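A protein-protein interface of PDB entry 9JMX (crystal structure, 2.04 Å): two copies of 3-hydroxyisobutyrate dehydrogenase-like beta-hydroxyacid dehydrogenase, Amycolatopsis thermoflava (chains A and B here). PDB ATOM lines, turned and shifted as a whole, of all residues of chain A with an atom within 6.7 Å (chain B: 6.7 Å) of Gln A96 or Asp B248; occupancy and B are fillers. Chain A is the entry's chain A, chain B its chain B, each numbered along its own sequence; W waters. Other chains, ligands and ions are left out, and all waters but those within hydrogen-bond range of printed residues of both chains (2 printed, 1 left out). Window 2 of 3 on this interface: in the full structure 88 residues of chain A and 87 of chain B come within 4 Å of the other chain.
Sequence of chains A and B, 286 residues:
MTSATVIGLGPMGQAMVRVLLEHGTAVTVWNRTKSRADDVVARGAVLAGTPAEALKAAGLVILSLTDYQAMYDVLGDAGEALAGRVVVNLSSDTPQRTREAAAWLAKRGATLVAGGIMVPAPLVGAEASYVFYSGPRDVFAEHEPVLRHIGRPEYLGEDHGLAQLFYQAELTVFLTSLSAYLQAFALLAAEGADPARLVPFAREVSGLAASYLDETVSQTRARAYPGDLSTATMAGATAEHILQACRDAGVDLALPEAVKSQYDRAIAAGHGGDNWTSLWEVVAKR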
ATOM      1  N   ASP A  93      32.466 -11.961  18.826  1.00  0.00           N
ATOM      2  CA  ASP A  93      31.298 -11.992  19.749  1.00  0.00           C
ATOM      3  C   ASP A  93      30.696 -13.380  19.631  1.00  0.00           C
ATOM      4  O   ASP A  93      31.326 -14.236  18.986  1.00  0.00           O
ATOM      5  CB  ASP A  93      30.259 -10.888  19.504  1.00  0.00           C
ATOM      6  CG  ASP A  93      29.706 -10.400  20.841  1.00  0.00           C
ATOM      7  OD1 ASP A  93      29.117 -11.226  21.583  1.00  0.00           O
ATOM      8  OD2 ASP A  93      29.998  -9.253  21.193  1.00  0.00           O
ATOM      9  N   THR A  94      29.560 -13.634  20.256  1.00  0.00           N
ATOM     10  CA  THR A  94      28.929 -14.962  20.151  1.00  0.00           C
ATOM     11  C   THR A  94      28.149 -15.041  18.850  1.00  0.00           C
ATOM     12  O   THR A  94      27.659 -14.033  18.333  1.00  0.00           O
ATOM     13  CB  THR A  94      28.046 -15.273  21.360  1.00  0.00           C
ATOM     14  OG1 THR A  94      26.921 -14.408  21.222  1.00  0.00           O
ATOM     15  CG2 THR A  94      28.784 -15.099  22.668  1.00  0.00           C
ATOM     16  N   PRO A  95      27.964 -16.260  18.311  1.00  0.00           N
ATOM     17  CA  PRO A  95      26.983 -16.479  17.247  1.00  0.00           C
ATOM     18  C   PRO A  95      25.604 -15.844  17.548  1.00  0.00           C
ATOM     19  O   PRO A  95      25.078 -15.154  16.666  1.00  0.00           O
ATOM     20  CB  PRO A  95      26.948 -18.009  17.173  1.00  0.00           C
ATOM     21  CG  PRO A  95      28.375 -18.392  17.481  1.00  0.00           C
ATOM     22  CD  PRO A  95      28.747 -17.466  18.622  1.00  0.00           C
ATOM     23  N   GLN A  96      25.017 -16.081  18.724  1.00  0.00           N
ATOM     24  CA  GLN A  96      23.649 -15.562  19.035  1.00  0.00           C
ATOM     25  C   GLN A  96      23.629 -14.028  18.990  1.00  0.00           C
ATOM     26  O   GLN A  96      22.656 -13.489  18.454  1.00  0.00           O
ATOM     27  CB  GLN A  96      23.080 -16.068  20.365  1.00  0.00           C
ATOM     28  CG  GLN A  96      22.601 -17.517  20.318  1.00  0.00           C
ATOM     29  CD  GLN A  96      21.540 -17.795  19.270  1.00  0.00           C
ATOM     30  OE1 GLN A  96      21.747 -17.657  18.051  1.00  0.00           O
ATOM     31  NE2 GLN A  96      20.392 -18.245  19.748  1.00  0.00           N
ATOM     32  N   ARG A  97      24.641 -13.342  19.501  1.00  0.00           N
ATOM     33  CA  ARG A  97      24.691 -11.854  19.457  1.00  0.00           C
ATOM     34  C   ARG A  97      24.908 -11.358  18.030  1.00  0.00           C
ATOM     35  O   ARG A  97      24.387 -10.264  17.719  1.00  0.00           O
ATOM     36  CB  ARG A  97      25.706 -11.327  20.464  1.00  0.00           C
ATOM     37  CG  ARG A  97      25.149 -11.526  21.867  1.00  0.00           C
ATOM     38  CD  ARG A  97      25.678 -10.688  22.994  1.00  0.00           C
ATOM     39  NE  ARG A  97      26.257  -9.387  22.712  1.00  0.00           N
ATOM     40  CZ  ARG A  97      25.695  -8.196  22.946  1.00  0.00           C
ATOM     41  NH1 ARG A  97      24.451  -8.081  23.383  1.00  0.00           N
ATOM     42  NH2 ARG A  97      26.411  -7.103  22.742  1.00  0.00           N
ATOM     43  N   THR A  98      25.594 -12.142  17.190  1.00  0.00           N
ATOM     44  CA  THR A  98      25.769 -11.839  15.745  1.00  0.00           C
ATOM     45  C   THR A  98      24.391 -11.906  15.058  1.00  0.00           C
ATOM     46  O   THR A  98      24.049 -10.964  14.332  1.00  0.00           O
ATOM     47  CB  THR A  98      26.816 -12.771  15.123  1.00  0.00           C
ATOM     48  OG1 THR A  98      28.033 -12.601  15.857  1.00  0.00           O
ATOM     49  CG2 THR A  98      27.039 -12.508  13.649  1.00  0.00           C
ATOM     50  N   ARG A  99      23.616 -12.960  15.307  1.00  0.00           N
ATOM     51  CA  ARG A  99      22.251 -13.134  14.740  1.00  0.00           C
ATOM     52  C   ARG A  99      21.345 -11.979  15.212  1.00  0.00           C
ATOM     53  O   ARG A  99      20.741 -11.306  14.348  1.00  0.00           O
ATOM     54  CB  ARG A  99      21.743 -14.522  15.105  1.00  0.00           C
ATOM     55  CG  ARG A  99      22.468 -15.612  14.341  1.00  0.00           C
ATOM     56  CD  ARG A  99      21.981 -16.991  14.720  1.00  0.00           C
ATOM     57  NE  ARG A  99      22.893 -18.018  14.237  1.00  0.00           N
ATOM     58  CZ  ARG A  99      23.509 -18.922  15.002  1.00  0.00           C
ATOM     59  NH1 ARG A  99      23.342 -18.941  16.310  1.00  0.00           N
ATOM     60  NH2 ARG A  99      24.312 -19.811  14.448  1.00  0.00           N
ATOM     61  N   GLU A 100      21.323 -11.677  16.514  1.00  0.00           N
ATOM     62  CA  GLU A 100      20.595 -10.497  17.056  1.00  0.00           C
ATOM     63  C   GLU A 100      21.014  -9.230  16.306  1.00  0.00           C
ATOM     64  O   GLU A 100      20.128  -8.404  15.974  1.00  0.00           O
ATOM     65  CB  GLU A 100      20.932 -10.205  18.511  1.00  0.00           C
ATOM     66  CG  GLU A 100      20.361 -11.187  19.488  1.00  0.00           C
ATOM     67  CD  GLU A 100      20.412 -10.626  20.899  1.00  0.00           C
ATOM     68  OE1 GLU A 100      19.882 -11.304  21.797  1.00  0.00           O
ATOM     69  OE2 GLU A 100      20.962  -9.490  21.082  1.00  0.00           O
ATOM     70  N   ALA A 101      22.320  -9.047  16.102  1.00  0.00           N
ATOM     71  CA  ALA A 101      22.863  -7.819  15.490  1.00  0.00           C
ATOM     72  C   ALA A 101      22.301  -7.663  14.066  1.00  0.00           C
ATOM     73  O   ALA A 101      21.966  -6.541  13.722  1.00  0.00           O
ATOM     74  CB  ALA A 101      24.364  -7.795  15.539  1.00  0.00           C
ATOM     75  N   GLY A 161      25.431 -15.989  11.933  1.00  0.00           N
ATOM     76  CA  GLY A 161      26.159 -16.607  13.061  1.00  0.00           C
ATOM     77  C   GLY A 161      27.317 -17.500  12.622  1.00  0.00           C
ATOM     78  O   GLY A 161      28.132 -17.862  13.505  1.00  0.00           O
ATOM     79  N   GLN A 164      31.016 -16.261  12.699  1.00  0.00           N
ATOM     80  CA  GLN A 164      31.285 -16.050  14.136  1.00  0.00           C
ATOM     81  C   GLN A 164      31.541 -17.402  14.812  1.00  0.00           C
ATOM     82  O   GLN A 164      32.491 -17.500  15.582  1.00  0.00           O
ATOM     83  CB  GLN A 164      30.107 -15.305  14.771  1.00  0.00           C
ATOM     84  CG  GLN A 164      30.472 -14.723  16.127  1.00  0.00           C
ATOM     85  CD  GLN A 164      31.442 -13.575  16.042  1.00  0.00           C
ATOM     86  OE1 GLN A 164      32.655 -13.744  16.158  1.00  0.00           O
ATOM     87  NE2 GLN A 164      30.902 -12.366  15.943  1.00  0.00           N
ATOM     88  N   GLU B 191      25.666 -26.310  17.311  1.00  0.00           N
ATOM     89  CA  GLU B 191      24.965 -25.279  16.494  1.00  0.00           C
ATOM     90  C   GLU B 191      24.573 -25.885  15.131  1.00  0.00           C
ATOM     91  O   GLU B 191      24.170 -25.123  14.233  1.00  0.00           O
ATOM     92  CB  GLU B 191      25.871 -24.055  16.336  1.00  0.00           C
ATOM     93  CG  GLU B 191      26.123 -23.307  17.637  1.00  0.00           C
ATOM     94  CD  GLU B 191      25.389 -21.980  17.803  1.00  0.00           C
ATOM     95  OE1 GLU B 191      25.215 -21.525  18.966  1.00  0.00           O
ATOM     96  OE2 GLU B 191      25.000 -21.401  16.782  1.00  0.00           O
ATOM     97  N   HIS B 241      33.850 -14.656  24.774  1.00  0.00           N
ATOM     98  CA  HIS B 241      32.902 -14.977  23.663  1.00  0.00           C
ATOM     99  C   HIS B 241      32.834 -16.499  23.508  1.00  0.00           C
ATOM    100  O   HIS B 241      31.709 -17.047  23.316  1.00  0.00           O
ATOM    101  CB  HIS B 241      33.254 -14.225  22.377  1.00  0.00           C
ATOM    102  CG  HIS B 241      33.289 -12.733  22.550  1.00  0.00           C
ATOM    103  ND1 HIS B 241      34.146 -11.927  21.830  1.00  0.00           N
ATOM    104  CD2 HIS B 241      32.592 -11.909  23.373  1.00  0.00           C
ATOM    105  CE1 HIS B 241      33.976 -10.660  22.195  1.00  0.00           C
ATOM    106  NE2 HIS B 241      33.009 -10.619  23.150  1.00  0.00           N
ATOM    107  N   LEU B 243      33.349 -18.824  25.912  1.00  0.00           N
ATOM    108  CA  LEU B 243      32.597 -19.364  27.067  1.00  0.00           C
ATOM    109  C   LEU B 243      31.111 -19.062  26.854  1.00  0.00           C
ATOM    110  O   LEU B 243      30.303 -19.969  27.079  1.00  0.00           O
ATOM    111  CB  LEU B 243      33.135 -18.709  28.344  1.00  0.00           C
ATOM    112  CG  LEU B 243      32.424 -19.009  29.661  1.00  0.00           C
ATOM    113  CD1 LEU B 243      32.585 -20.460  30.062  1.00  0.00           C
ATOM    114  CD2 LEU B 243      33.011 -18.151  30.745  1.00  0.00           C
ATOM    115  N   GLN B 244      30.764 -17.830  26.465  1.00  0.00           N
ATOM    116  CA  GLN B 244      29.350 -17.455  26.202  1.00  0.00           C
ATOM    117  C   GLN B 244      28.768 -18.276  25.036  1.00  0.00           C
ATOM    118  O   GLN B 244      27.628 -18.744  25.189  1.00  0.00           O
ATOM    119  CB  GLN B 244      29.239 -15.953  25.947  1.00  0.00           C
ATOM    120  CG  GLN B 244      29.583 -15.115  27.171  1.00  0.00           C
ATOM    121  CD  GLN B 244      29.604 -13.635  26.880  1.00  0.00           C
ATOM    122  OE1 GLN B 244      29.714 -13.211  25.741  1.00  0.00           O
ATOM    123  NE2 GLN B 244      29.499 -12.835  27.922  1.00  0.00           N
ATOM    124  N   ALA B 245      29.486 -18.433  23.909  1.00  0.00           N
ATOM    125  CA  ALA B 245      29.035 -19.266  22.755  1.00  0.00           C
ATOM    126  C   ALA B 245      28.782 -20.702  23.220  1.00  0.00           C
ATOM    127  O   ALA B 245      27.702 -21.268  22.892  1.00  0.00           O
ATOM    128  CB  ALA B 245      30.014 -19.245  21.610  1.00  0.00           C
ATOM    129  N   CYS B 246      29.702 -21.272  24.000  1.00  0.00           N
ATOM    130  CA  CYS B 246      29.558 -22.654  24.507  1.00  0.00           C
ATOM    131  C   CYS B 246      28.351 -22.722  25.455  1.00  0.00           C
ATOM    132  O   CYS B 246      27.617 -23.731  25.424  1.00  0.00           O
ATOM    133  CB  CYS B 246      30.863 -23.137  25.141  1.00  0.00           C
ATOM    134  SG  CYS B 246      32.177 -23.415  23.920  1.00  0.00           S
ATOM    135  N   ARG B 247      28.207 -21.751  26.354  1.00  0.00           N
ATOM    136  CA  ARG B 247      27.066 -21.692  27.312  1.00  0.00           C
ATOM    137  C   ARG B 247      25.757 -21.703  26.492  1.00  0.00           C
ATOM    138  O   ARG B 247      24.876 -22.510  26.792  1.00  0.00           O
ATOM    139  CB  ARG B 247      27.220 -20.441  28.188  1.00  0.00           C
ATOM    140  CG  ARG B 247      26.004 -20.086  29.037  1.00  0.00           C
ATOM    141  CD  ARG B 247      26.033 -18.603  29.353  1.00  0.00           C
ATOM    142  NE  ARG B 247      25.803 -17.858  28.133  1.00  0.00           N
ATOM    143  CZ  ARG B 247      25.898 -16.546  28.011  1.00  0.00           C
ATOM    144  NH1 ARG B 247      25.639 -15.981  26.846  1.00  0.00           N
ATOM    145  NH2 ARG B 247      26.244 -15.798  29.049  1.00  0.00           N
ATOM    146  N   ASP B 248      25.661 -20.846  25.478  1.00  0.00           N
ATOM    147  CA  ASP B 248      24.491 -20.734  24.564  1.00  0.00           C
ATOM    148  C   ASP B 248      24.207 -22.081  23.874  1.00  0.00           C
ATOM    149  O   ASP B 248      23.020 -22.495  23.819  1.00  0.00           O
ATOM    150  CB  ASP B 248      24.707 -19.631  23.542  1.00  0.00           C
ATOM    151  CG  ASP B 248      24.782 -18.226  24.112  1.00  0.00           C
ATOM    152  OD1 ASP B 248      24.531 -18.058  25.351  1.00  0.00           O
ATOM    153  OD2 ASP B 248      25.114 -17.307  23.331  1.00  0.00           O
ATOM    154  N   ALA B 249      25.226 -22.806  23.417  1.00  0.00           N
ATOM    155  CA  ALA B 249      25.020 -24.040  22.623  1.00  0.00           C
ATOM    156  C   ALA B 249      24.888 -25.284  23.519  1.00  0.00           C
ATOM    157  O   ALA B 249      24.651 -26.373  22.981  1.00  0.00           O
ATOM    158  CB  ALA B 249      26.138 -24.160  21.620  1.00  0.00           C
ATOM    159  N   GLY B 250      25.019 -25.152  24.839  1.00  0.00           N
ATOM    160  CA  GLY B 250      24.922 -26.280  25.778  1.00  0.00           C
ATOM    161  C   GLY B 250      26.167 -27.176  25.806  1.00  0.00           C
ATOM    162  O   GLY B 250      26.032 -28.367  26.135  1.00  0.00           O
ATOM    163  N   VAL B 251      27.340 -26.632  25.499  1.00  0.00           N
ATOM    164  CA  VAL B 251      28.643 -27.358  25.497  1.00  0.00           C
ATOM    165  C   VAL B 251      29.286 -27.158  26.871  1.00  0.00           C
ATOM    166  O   VAL B 251      29.052 -26.089  27.490  1.00  0.00           O
ATOM    167  CB  VAL B 251      29.519 -26.831  24.342  1.00  0.00           C
ATOM    168  CG1 VAL B 251      30.958 -27.296  24.411  1.00  0.00           C
ATOM    169  CG2 VAL B 251      28.907 -27.205  23.005  1.00  0.00           C
ATOM    170  N   LEU B 253      31.620 -26.016  29.788  1.00  0.00           N
ATOM    171  CA  LEU B 253      32.291 -24.706  29.957  1.00  0.00           C
ATOM    172  C   LEU B 253      33.644 -24.850  30.648  1.00  0.00           C
ATOM    173  O   LEU B 253      34.320 -23.839  30.741  1.00  0.00           O
ATOM    174  CB  LEU B 253      31.368 -23.782  30.758  1.00  0.00           C
ATOM    175  CG  LEU B 253      30.032 -23.522  30.073  1.00  0.00           C
ATOM    176  CD1 LEU B 253      29.297 -22.384  30.715  1.00  0.00           C
ATOM    177  CD2 LEU B 253      30.225 -23.254  28.589  1.00  0.00           C
HETATM  178  O   HOH W   1      25.866 -17.938  20.730  1.00  0.00           O
HETATM  179  O   HOH W   2      29.019 -11.246  24.121  1.00  0.00           O
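Among the printed residues, pairs that only touch across the chains: Thr A94 with Gln B244 (3.4 Å), Thr A94 with His B241 (3.6 Å), Thr A94 with Ala B245 (3.6 Å), Pro A95 with Ala B245 (3.7 Å), Gln A96 with Asp B248 (3.8 Å) and Pro A95 with Glu B191 (3.9 Å).
OG1 of Thr A94 sits at hydrogen-bond distance from N of Arg A97, 3.0 Å away. The side-chain carboxylate of Asp A93 lies within salt-bridge range of the guanidinium group of Arg A97 (3.6 Å). The side-chain carboxylate (OD1) of Asp B248 lies within salt-bridge range of the guanidinium group (NH1) of Arg B247 (2.8 Å). The backbone carbonyl oxygen of Thr A94 is in hydrogen-bond range of the side-chain hydroxyl of Thr A98. The side-chain amide oxygen (OE1) of Gln A96 is in hydrogen-bond range of the guanidinium group (NH1) of Arg A99, at 2.7 Å. OE1 of Gln A164 sits close to O of Asp A93 (3.2 Å).
Of the printed residues of chain B, Thr A94 touches His B241 (3.6 Å), Gln B244 (3.4 Å) and Ala B245 (3.6 Å). Of chain B, only Asp B248 comes within 4 Å of Gln A96. Printed residues of chain A within 4 Å of Glu B191: Pro A95 and Arg A99. Leu B243 touches none of the printed residues of chain A. Of the printed residues of chain A, Gln B244 touches Thr A94 (3.4 Å). Of the printed residues of chain A, Asp B248 touches Gln A96. The nearest residue of chain B that does not touch Gln A96 is Glu B191 (5.0 Å). The nearest printed residue of chain A that does not touch Ala B245 is Asp A93 (5.8 Å).
A ring nitrogen (ND1) of His B241 is in hydrogen-bond range of the backbone NH of Asp A93 (3.4 Å). NH2 of Arg A99 lies within salt-bridge range of OE2 of Glu B191, 2.9 Å away.
Water W2 lies within hydrogen-bond range of the side-chain carboxylate of Asp A93 and the side-chain amide oxygen of Gln B244. Water W1 bridges the side-chain carboxylate (OD2) of Asp B248 and the backbone NH (N) of Gln A96.
Of the 11 printed residues of chain A, 5 touch a printed residue of chain B. Hydrophobic or aromatic side chains of chain A that line the printed part of chain B: Pro A95. Along chain B the printed residues that touch a printed residue of chain A span positions 191 to 248. Among the printed residues, 8 pairs touch across the chains. Among the printed residues, Asp or Glu carboxylates within 4 Å of a Lys or Arg side-chain nitrogen of the other chain: Arg A99 with Glu B191 (2.9 Å).
No position is printed for both chains.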
